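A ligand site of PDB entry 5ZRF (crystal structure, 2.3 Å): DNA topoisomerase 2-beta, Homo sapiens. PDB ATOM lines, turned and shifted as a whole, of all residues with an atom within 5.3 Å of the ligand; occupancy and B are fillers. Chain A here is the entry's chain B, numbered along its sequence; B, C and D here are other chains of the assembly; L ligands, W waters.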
ATOM      1  N   GLU A  59      -8.527  19.567  -0.598  1.00  0.00           N
ATOM      2  CA  GLU A  59      -8.060  18.524   0.299  1.00  0.00           C
ATOM      3  C   GLU A  59      -6.804  19.088   0.955  1.00  0.00           C
ATOM      4  O   GLU A  59      -5.706  18.999   0.387  1.00  0.00           O
ATOM      5  CB  GLU A  59      -7.779  17.239  -0.473  1.00  0.00           C
ATOM      6  CG  GLU A  59      -6.947  16.169   0.244  1.00  0.00           C
ATOM      7  CD  GLU A  59      -6.893  14.830  -0.522  1.00  0.00           C
ATOM      8  OE1 GLU A  59      -6.561  13.787   0.071  1.00  0.00           O
ATOM      9  OE2 GLU A  59      -7.227  14.833  -1.735  1.00  0.00           O
ATOM     10  N   GLY A  60      -6.936  19.579   2.189  1.00  0.00           N
ATOM     11  CA  GLY A  60      -5.809  20.057   2.952  1.00  0.00           C
ATOM     12  C   GLY A  60      -5.468  21.517   2.703  1.00  0.00           C
ATOM     13  O   GLY A  60      -5.878  22.135   1.722  1.00  0.00           O
ATOM     14  N   ASP A  61      -4.657  22.064   3.613  1.00  0.00           N
ATOM     15  CA  ASP A  61      -4.337  23.486   3.577  1.00  0.00           C
ATOM     16  C   ASP A  61      -3.380  23.828   2.449  1.00  0.00           C
ATOM     17  O   ASP A  61      -3.524  24.868   1.794  1.00  0.00           O
ATOM     18  CB  ASP A  61      -3.770  23.944   4.926  1.00  0.00           C
ATOM     19  CG  ASP A  61      -4.763  23.761   6.076  1.00  0.00           C
ATOM     20  OD1 ASP A  61      -5.771  24.497   6.104  1.00  0.00           O
ATOM     21  OD2 ASP A  61      -4.529  22.877   6.932  1.00  0.00           O
ATOM     22  N   LEU A  84     -10.443  21.379   3.487  1.00  0.00           N
ATOM     23  CA  LEU A  84     -10.930  20.230   4.226  1.00  0.00           C
ATOM     24  C   LEU A  84      -9.746  19.555   4.905  1.00  0.00           C
ATOM     25  O   LEU A  84      -8.634  19.534   4.380  1.00  0.00           O
ATOM     26  CB  LEU A  84     -11.646  19.241   3.307  1.00  0.00           C
ATOM     27  CG  LEU A  84     -12.896  19.742   2.598  1.00  0.00           C
ATOM     28  CD1 LEU A  84     -13.362  18.711   1.583  1.00  0.00           C
ATOM     29  CD2 LEU A  84     -14.038  20.060   3.580  1.00  0.00           C
ATOM     30  N   ARG A  85     -10.009  18.996   6.076  1.00  0.00           N
ATOM     31  CA  ARG A  85      -9.033  18.362   6.945  1.00  0.00           C
ATOM     32  C   ARG A  85      -8.802  16.898   6.594  1.00  0.00           C
ATOM     33  O   ARG A  85      -8.400  16.131   7.464  1.00  0.00           O
ATOM     34  CB  ARG A  85      -9.455  18.481   8.410  1.00  0.00           C
ATOM     35  CG  ARG A  85      -9.374  19.896   8.947  1.00  0.00           C
ATOM     36  CD  ARG A  85      -9.452  19.922  10.467  1.00  0.00           C
ATOM     37  NE  ARG A  85     -10.666  19.327  11.000  1.00  0.00           N
ATOM     38  CZ  ARG A  85     -11.066  19.480  12.262  1.00  0.00           C
ATOM     39  NH1 ARG A  85     -10.318  20.199  13.091  1.00  0.00           N
ATOM     40  NH2 ARG A  85     -12.182  18.912  12.698  1.00  0.00           N
ATOM     41  N   GLY A  86      -9.131  16.463   5.381  1.00  0.00           N
ATOM     42  CA  GLY A  86      -9.149  15.038   5.112  1.00  0.00           C
ATOM     43  C   GLY A  86     -10.553  14.458   5.051  1.00  0.00           C
ATOM     44  O   GLY A  86     -11.447  15.088   4.473  1.00  0.00           O
ATOM     45  N   GLN A 360       3.468   9.879   8.144  1.00  0.00           N
ATOM     46  CA  GLN A 360       3.024   9.699   9.527  1.00  0.00           C
ATOM     47  C   GLN A 360       2.272   8.385   9.707  1.00  0.00           C
ATOM     48  O   GLN A 360       2.448   7.703  10.725  1.00  0.00           O
ATOM     49  CB  GLN A 360       2.183  10.907   9.973  1.00  0.00           C
ATOM     50  CG  GLN A 360       1.042  11.296   9.034  1.00  0.00           C
ATOM     51  CD  GLN A 360      -0.180  10.437   9.214  1.00  0.00           C
ATOM     52  OE1 GLN A 360      -0.444   9.934  10.312  1.00  0.00           O
ATOM     53  NE2 GLN A 360      -0.926  10.224   8.133  1.00  0.00           N
ATOM     54  N   MET A 364       3.259   5.257  12.300  1.00  0.00           N
ATOM     55  CA  MET A 364       2.344   4.508  13.139  1.00  0.00           C
ATOM     56  C   MET A 364       2.403   3.011  12.818  1.00  0.00           C
ATOM     57  O   MET A 364       2.452   2.176  13.725  1.00  0.00           O
ATOM     58  CB  MET A 364       0.916   5.041  12.986  1.00  0.00           C
ATOM     59  CG  MET A 364       0.746   6.486  13.453  1.00  0.00           C
ATOM     60  SD  MET A 364      -0.974   7.103  13.461  1.00  0.00           S
ATOM     61  CE  MET A 364      -1.687   6.191  14.839  1.00  0.00           C
ATOM     62  N   PRO A 401       7.452   9.463  17.116  1.00  0.00           N
ATOM     63  CA  PRO A 401       8.348   8.702  16.227  1.00  0.00           C
ATOM     64  C   PRO A 401       9.670   9.413  15.972  1.00  0.00           C
ATOM     65  O   PRO A 401      10.604   8.797  15.449  1.00  0.00           O
ATOM     66  CB  PRO A 401       7.538   8.525  14.937  1.00  0.00           C
ATOM     67  CG  PRO A 401       6.487   9.582  15.004  1.00  0.00           C
ATOM     68  CD  PRO A 401       6.188   9.819  16.448  1.00  0.00           C
ATOM     69  P    DA B   4      -6.002  15.516  22.466  1.00  0.00           P
ATOM     70  OP1  DA B   4      -6.930  15.483  23.624  1.00  0.00           O
ATOM     71  OP2  DA B   4      -5.122  14.362  22.167  1.00  0.00           O
ATOM     72  O5'  DA B   4      -6.854  15.811  21.155  1.00  0.00           O
ATOM     73  C5'  DA B   4      -7.736  16.914  21.107  1.00  0.00           C
ATOM     74  C4'  DA B   4      -8.168  17.153  19.682  1.00  0.00           C
ATOM     75  O4'  DA B   4      -7.030  17.633  18.932  1.00  0.00           O
ATOM     76  C3'  DA B   4      -8.653  15.898  18.956  1.00  0.00           C
ATOM     77  O3'  DA B   4     -10.070  15.736  19.126  1.00  0.00           O
ATOM     78  C2'  DA B   4      -8.271  16.172  17.497  1.00  0.00           C
ATOM     79  C1'  DA B   4      -7.021  17.053  17.631  1.00  0.00           C
ATOM     80  N9   DA B   4      -5.754  16.331  17.443  1.00  0.00           N
ATOM     81  C8   DA B   4      -5.339  15.195  18.084  1.00  0.00           C
ATOM     82  N7   DA B   4      -4.144  14.773  17.701  1.00  0.00           N
ATOM     83  C5   DA B   4      -3.764  15.680  16.744  1.00  0.00           C
ATOM     84  C6   DA B   4      -2.615  15.788  15.935  1.00  0.00           C
ATOM     85  N6   DA B   4      -1.597  14.924  15.999  1.00  0.00           N
ATOM     86  N1   DA B   4      -2.543  16.820  15.060  1.00  0.00           N
ATOM     87  C2   DA B   4      -3.563  17.687  15.009  1.00  0.00           C
ATOM     88  N3   DA B   4      -4.702  17.687  15.711  1.00  0.00           N
ATOM     89  C4   DA B   4      -4.741  16.655  16.569  1.00  0.00           C
ATOM     90  P    DG B   5     -10.779  14.352  18.734  1.00  0.00           P
ATOM     91  OP1  DG B   5     -11.942  14.123  19.609  1.00  0.00           O
ATOM     92  OP2  DG B   5      -9.701  13.332  18.647  1.00  0.00           O
ATOM     93  O5'  DG B   5     -11.337  14.608  17.251  1.00  0.00           O
ATOM     94  C5'  DG B   5     -12.236  15.683  17.009  1.00  0.00           C
ATOM     95  C4'  DG B   5     -12.566  15.790  15.528  1.00  0.00           C
ATOM     96  O4'  DG B   5     -11.370  16.163  14.790  1.00  0.00           O
ATOM     97  C3'  DG B   5     -13.042  14.511  14.868  1.00  0.00           C
ATOM     98  O3'  DG B   5     -14.449  14.353  15.038  1.00  0.00           O
ATOM     99  C2'  DG B   5     -12.705  14.790  13.409  1.00  0.00           C
ATOM    100  C1'  DG B   5     -11.367  15.519  13.527  1.00  0.00           C
ATOM    101  N9   DG B   5     -10.213  14.626  13.433  1.00  0.00           N
ATOM    102  C8   DG B   5      -9.465  14.133  14.479  1.00  0.00           C
ATOM    103  N7   DG B   5      -8.509  13.334  14.085  1.00  0.00           N
ATOM    104  C5   DG B   5      -8.628  13.303  12.695  1.00  0.00           C
ATOM    105  C6   DG B   5      -7.857  12.608  11.729  1.00  0.00           C
ATOM    106  O6   DG B   5      -6.887  11.874  11.917  1.00  0.00           O
ATOM    107  N1   DG B   5      -8.310  12.837  10.429  1.00  0.00           N
ATOM    108  C2   DG B   5      -9.395  13.644  10.119  1.00  0.00           C
ATOM    109  N2   DG B   5      -9.707  13.749   8.817  1.00  0.00           N
ATOM    110  N3   DG B   5     -10.116  14.300  11.021  1.00  0.00           N
ATOM    111  C4   DG B   5      -9.676  14.077  12.282  1.00  0.00           C
ATOM    112  P    DC B   6     -15.133  12.896  14.947  1.00  0.00           P
ATOM    113  OP1  DC B   6     -16.589  13.075  15.085  1.00  0.00           O
ATOM    114  OP2  DC B   6     -14.388  11.990  15.846  1.00  0.00           O
ATOM    115  O5'  DC B   6     -14.812  12.384  13.457  1.00  0.00           O
ATOM    116  C5'  DC B   6     -15.530  12.888  12.354  1.00  0.00           C
ATOM    117  C4'  DC B   6     -14.909  12.403  11.058  1.00  0.00           C
ATOM    118  O4'  DC B   6     -13.482  12.632  11.115  1.00  0.00           O
ATOM    119  C3'  DC B   6     -15.031  10.918  10.791  1.00  0.00           C
ATOM    120  O3'  DC B   6     -16.253  10.650  10.168  1.00  0.00           O
ATOM    121  C2'  DC B   6     -13.881  10.681   9.825  1.00  0.00           C
ATOM    122  C1'  DC B   6     -12.834  11.686  10.284  1.00  0.00           C
ATOM    123  N1   DC B   6     -11.717  11.086  11.038  1.00  0.00           N
ATOM    124  C2   DC B   6     -10.720  10.383  10.353  1.00  0.00           C
ATOM    125  O2   DC B   6     -10.816  10.266   9.121  1.00  0.00           O
ATOM    126  N3   DC B   6      -9.700   9.835  11.052  1.00  0.00           N
ATOM    127  C4   DC B   6      -9.637   9.973  12.371  1.00  0.00           C
ATOM    128  N4   DC B   6      -8.610   9.436  13.016  1.00  0.00           N
ATOM    129  C5   DC B   6     -10.651  10.686  13.087  1.00  0.00           C
ATOM    130  C6   DC B   6     -11.664  11.221  12.392  1.00  0.00           C
ATOM    131  P    DG C   7      -1.477   2.317   4.197  1.00  0.00           P
ATOM    132  OP1  DG C   7      -1.236   1.395   3.072  1.00  0.00           O
ATOM    133  OP2  DG C   7      -0.379   2.808   5.042  1.00  0.00           O
ATOM    134  O5'  DG C   7      -2.254   3.582   3.593  1.00  0.00           O
ATOM    135  C5'  DG C   7      -2.298   4.826   4.296  1.00  0.00           C
ATOM    136  C4'  DG C   7      -3.671   5.454   4.193  1.00  0.00           C
ATOM    137  O4'  DG C   7      -4.465   5.088   5.356  1.00  0.00           O
ATOM    138  C3'  DG C   7      -3.692   6.982   4.203  1.00  0.00           C
ATOM    139  O3'  DG C   7      -3.458   7.487   2.894  1.00  0.00           O
ATOM    140  C2'  DG C   7      -5.125   7.268   4.655  1.00  0.00           C
ATOM    141  C1'  DG C   7      -5.399   6.117   5.636  1.00  0.00           C
ATOM    142  N9   DG C   7      -5.294   6.532   7.045  1.00  0.00           N
ATOM    143  C8   DG C   7      -4.211   6.405   7.903  1.00  0.00           C
ATOM    144  N7   DG C   7      -4.458   6.886   9.110  1.00  0.00           N
ATOM    145  C5   DG C   7      -5.768   7.369   9.022  1.00  0.00           C
ATOM    146  C6   DG C   7      -6.591   8.007   9.980  1.00  0.00           C
ATOM    147  O6   DG C   7      -6.319   8.301  11.155  1.00  0.00           O
ATOM    148  N1   DG C   7      -7.842   8.327   9.463  1.00  0.00           N
ATOM    149  C2   DG C   7      -8.254   8.061   8.182  1.00  0.00           C
ATOM    150  N2   DG C   7      -9.484   8.449   7.856  1.00  0.00           N
ATOM    151  N3   DG C   7      -7.496   7.469   7.284  1.00  0.00           N
ATOM    152  C4   DG C   7      -6.281   7.160   7.757  1.00  0.00           C
ATOM    153  P    DC C   8      -2.766   8.918   2.684  1.00  0.00           P
ATOM    154  OP1  DC C   8      -2.410   9.023   1.257  1.00  0.00           O
ATOM    155  OP2  DC C   8      -1.718   9.114   3.706  1.00  0.00           O
ATOM    156  O5'  DC C   8      -3.929   9.966   3.032  1.00  0.00           O
ATOM    157  C5'  DC C   8      -5.006  10.132   2.135  1.00  0.00           C
ATOM    158  C4'  DC C   8      -5.973  11.174   2.657  1.00  0.00           C
ATOM    159  O4'  DC C   8      -6.659  10.636   3.812  1.00  0.00           O
ATOM    160  C3'  DC C   8      -5.336  12.441   3.187  1.00  0.00           C
ATOM    161  O3'  DC C   8      -5.037  13.338   2.126  1.00  0.00           O
ATOM    162  C2'  DC C   8      -6.444  12.988   4.065  1.00  0.00           C
ATOM    163  C1'  DC C   8      -7.017  11.716   4.677  1.00  0.00           C
ATOM    164  N1   DC C   8      -6.520  11.430   6.042  1.00  0.00           N
ATOM    165  C2   DC C   8      -7.284  11.853   7.129  1.00  0.00           C
ATOM    166  O2   DC C   8      -8.354  12.442   6.920  1.00  0.00           O
ATOM    167  N3   DC C   8      -6.844  11.605   8.388  1.00  0.00           N
ATOM    168  C4   DC C   8      -5.695  10.959   8.584  1.00  0.00           C
ATOM    169  N4   DC C   8      -5.304  10.748   9.850  1.00  0.00           N
ATOM    170  C5   DC C   8      -4.879  10.520   7.479  1.00  0.00           C
ATOM    171  C6   DC C   8      -5.324  10.779   6.238  1.00  0.00           C
ATOM    172  P    IU D   1       1.653  15.578   5.707  1.00  0.00           P
ATOM    173  OP1  IU D   1       1.308  14.676   4.529  1.00  0.00           O
ATOM    174  OP2  IU D   1       2.724  14.928   6.571  1.00  0.00           O
ATOM    175  O5'  IU D   1       0.265  15.811   6.628  1.00  0.00           O
ATOM    176  C5'  IU D   1      -0.789  16.488   5.981  1.00  0.00           C
ATOM    177  C4'  IU D   1      -1.188  17.656   6.957  1.00  0.00           C
ATOM    178  O4'  IU D   1      -1.343  16.965   8.302  1.00  0.00           O
ATOM    179  C3'  IU D   1      -0.254  18.535   7.109  1.00  0.00           C
ATOM    180  O3'  IU D   1      -0.697  19.785   6.487  1.00  0.00           O
ATOM    181  C2'  IU D   1      -0.086  18.766   8.742  1.00  0.00           C
ATOM    182  C1'  IU D   1      -1.036  18.114   9.295  1.00  0.00           C
ATOM    183  N1   IU D   1      -0.586  17.394  10.513  1.00  0.00           N
ATOM    184  C2   IU D   1      -1.416  17.434  11.746  1.00  0.00           C
ATOM    185  O2   IU D   1      -2.416  18.052  11.768  1.00  0.00           O
ATOM    186  N3   IU D   1      -0.967  16.690  12.963  1.00  0.00           N
ATOM    187  C4   IU D   1       0.262  15.924  12.920  1.00  0.00           C
ATOM    188  O4   IU D   1       0.607  15.332  13.894  1.00  0.00           O
ATOM    189  C5   IU D   1       1.077  15.894  11.661  1.00  0.00           C
ATOM    190  C6   IU D   1       0.628  16.637  10.466  1.00  0.00           C
ATOM    191  I5   IU D   1       2.908  14.827  11.545  1.00  0.00           I
ATOM    192  P    DG D   2       0.301  21.036   6.282  1.00  0.00           P
ATOM    193  OP1  DG D   2      -0.070  21.556   4.955  1.00  0.00           O
ATOM    194  OP2  DG D   2       1.706  20.677   6.564  1.00  0.00           O
ATOM    195  O5'  DG D   2      -0.160  22.062   7.426  1.00  0.00           O
ATOM    196  C5'  DG D   2      -1.536  22.256   7.659  1.00  0.00           C
ATOM    197  C4'  DG D   2      -1.777  23.095   8.901  1.00  0.00           C
ATOM    198  O4'  DG D   2      -1.602  22.281  10.091  1.00  0.00           O
ATOM    199  C3'  DG D   2      -0.848  24.288   9.069  1.00  0.00           C
ATOM    200  O3'  DG D   2      -1.587  25.355   9.615  1.00  0.00           O
ATOM    201  C2'  DG D   2       0.217  23.771  10.037  1.00  0.00           C
ATOM    202  C1'  DG D   2      -0.619  22.863  10.927  1.00  0.00           C
ATOM    203  N9   DG D   2       0.128  21.766  11.544  1.00  0.00           N
ATOM    204  C8   DG D   2       1.197  21.092  11.009  1.00  0.00           C
ATOM    205  N7   DG D   2       1.622  20.126  11.771  1.00  0.00           N
ATOM    206  C5   DG D   2       0.762  20.141  12.859  1.00  0.00           C
ATOM    207  C6   DG D   2       0.729  19.306  14.013  1.00  0.00           C
ATOM    208  O6   DG D   2       1.478  18.373  14.302  1.00  0.00           O
ATOM    209  N1   DG D   2      -0.310  19.670  14.873  1.00  0.00           N
ATOM    210  C2   DG D   2      -1.197  20.691  14.646  1.00  0.00           C
ATOM    211  N2   DG D   2      -2.135  20.894  15.596  1.00  0.00           N
ATOM    212  N3   DG D   2      -1.173  21.468  13.579  1.00  0.00           N
ATOM    213  C4   DG D   2      -0.168  21.133  12.730  1.00  0.00           C
HETATM  214  C1  LIG L   1      -8.538  17.737  14.069  1.00  0.00           C
HETATM  215  O1  LIG L   1      -7.502  16.840  14.490  1.00  0.00           O
HETATM  216  C2  LIG L   1      -7.708  16.679  12.203  1.00  0.00           C
HETATM  217  O2  LIG L   1      -8.834  17.310  12.704  1.00  0.00           O
HETATM  218  C3  LIG L   1      -7.305  16.322  10.846  1.00  0.00           C
HETATM  219  O3  LIG L   1      -2.315  13.678   8.404  1.00  0.00           O
HETATM  220  C4  LIG L   1      -6.129  15.711  10.655  1.00  0.00           C
HETATM  221  O4  LIG L   1      -4.246  13.932   6.903  1.00  0.00           O
HETATM  222  C5  LIG L   1      -5.595  15.288   9.133  1.00  0.00           C
HETATM  223  O5  LIG L   1      -4.145  20.189   8.937  1.00  0.00           O
HETATM  224  C6  LIG L   1      -4.460  14.288   9.057  1.00  0.00           C
HETATM  225  O6  LIG L   1      -4.378  20.157   6.298  1.00  0.00           O
HETATM  226  C7  LIG L   1      -3.851  13.995   8.012  1.00  0.00           C
HETATM  227  O7  LIG L   1      -5.181  17.865   4.879  1.00  0.00           O
HETATM  228  C8  LIG L   1      -2.190  13.938   9.958  1.00  0.00           C
HETATM  229  O8  LIG L   1      -4.060  13.270  11.974  1.00  0.00           O
HETATM  230  C9  LIG L   1      -3.212  14.668  10.272  1.00  0.00           C
HETATM  231  O9  LIG L   1      -1.937  12.667  12.670  1.00  0.00           O
HETATM  232  C10 LIG L   1      -3.730  14.608  11.652  1.00  0.00           C
HETATM  233  O10 LIG L   1       1.133  11.265  14.361  1.00  0.00           O
HETATM  234  C11 LIG L   1      -5.181  15.397  11.924  1.00  0.00           C
HETATM  235  O11 LIG L   1      -0.880  10.132  15.248  1.00  0.00           O
HETATM  236  C12 LIG L   1      -5.565  15.715  13.154  1.00  0.00           C
HETATM  237  O12 LIG L   1      -3.622   9.439  14.760  1.00  0.00           O
HETATM  238  C13 LIG L   1      -6.849  16.376  13.348  1.00  0.00           C
HETATM  239  O13 LIG L   1      -5.283  11.765  14.007  1.00  0.00           O
HETATM  240  C14 LIG L   1      -5.239  16.638   8.400  1.00  0.00           C
HETATM  241  C15 LIG L   1      -4.849  17.789   9.080  1.00  0.00           C
HETATM  242  C16 LIG L   1      -4.555  18.980   8.357  1.00  0.00           C
HETATM  243  C17 LIG L   1      -4.670  18.988   6.987  1.00  0.00           C
HETATM  244  C18 LIG L   1      -5.065  17.849   6.303  1.00  0.00           C
HETATM  245  C19 LIG L   1      -5.351  16.693   6.997  1.00  0.00           C
HETATM  246  C20 LIG L   1      -4.479  20.411  10.278  1.00  0.00           C
HETATM  247  C21 LIG L   1      -5.092  16.589   4.220  1.00  0.00           C
HETATM  248  C22 LIG L   1      -3.372  12.837  13.063  1.00  0.00           C
HETATM  249  C23 LIG L   1      -1.105  12.027  13.771  1.00  0.00           C
HETATM  250  C24 LIG L   1       0.289  11.905  13.331  1.00  0.00           C
HETATM  251  C25 LIG L   1       0.564   9.989  14.878  1.00  0.00           C
HETATM  252  C26 LIG L   1      -1.673  10.679  14.182  1.00  0.00           C
HETATM  253  C27 LIG L   1      -3.135  10.760  14.558  1.00  0.00           C
HETATM  254  C28 LIG L   1      -3.975  11.492  13.506  1.00  0.00           C
HETATM  255  C29 LIG L   1       1.302   9.612  16.055  1.00  0.00           C
HETATM  256  O   HOH W   1       3.218   9.081  13.405  1.00  0.00           O
HETATM  257  O   HOH W   2      -2.652   8.510  17.275  1.00  0.00           O
HETATM  258  O   HOH W   3      -4.306   7.623  12.877  1.00  0.00           O
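Water W3 lies within hydrogen-bond range of O12 of the ligand (2.7 Å), O6 of DG 7 of chain C (2.7 Å) and SD of Met 364 (3.4 Å). Water W1 bridges the backbone carbonyl oxygen of Gln 360 (3.1 Å) and an oxygen (O10) of the ligand (3.2 Å).
N3 of DA 4 of chain B sits close to O1 of the ligand (3.2 Å). N1 of DC 8 of chain C lies close to O4 of the ligand (3.5 Å). O4' of IU 1 of chain D lies close to an oxygen (O3) of the ligand (3.4 Å). O4' of DG 2 of chain D sits close to an oxygen (O5) of the ligand (3.5 Å). Residues that only touch the ligand: Gly 60, Leu 84 and Gln 360. Of the 16 residues printed, 11 come within 4 Å of the ligand. The nearest printed residue that does not touch the ligand is Gly 86 (4.1 Å).
O6 of DG 5 of chain B lies within hydrogen-bond range of an oxygen (O13) of the ligand (2.6 Å). O6 of the ligand sits at hydrogen-bond distance from N of Asp 61 (3.3 Å). The side-chain carboxylate of Asp 61 lies within hydrogen-bond range of an oxygen (O6) of the ligand (2.8 Å). An oxygen (O2) of the ligand sits close to the guanidinium group (NE) of Arg 85 (3.2 Å). The side-chain sulfur (SD) of Met 364 lies close to an oxygen (O12) of the ligand (3.8 Å).
N2 of DG 5 of chain B sits close to O2 of DC 8 of chain C, 2.7 Å away. The backbone carbonyl oxygen (O) of Leu 84 sits at hydrogen-bond distance from the backbone NH (N) of Gly 60, at 2.8 Å. N3 of IU 1 of chain D lies close to N1 of DA 4 of chain B (2.6 Å). O3' of DC 8 of chain C sits close to the side-chain carboxylate (OE1) of Glu 59, 2.6 Å away.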
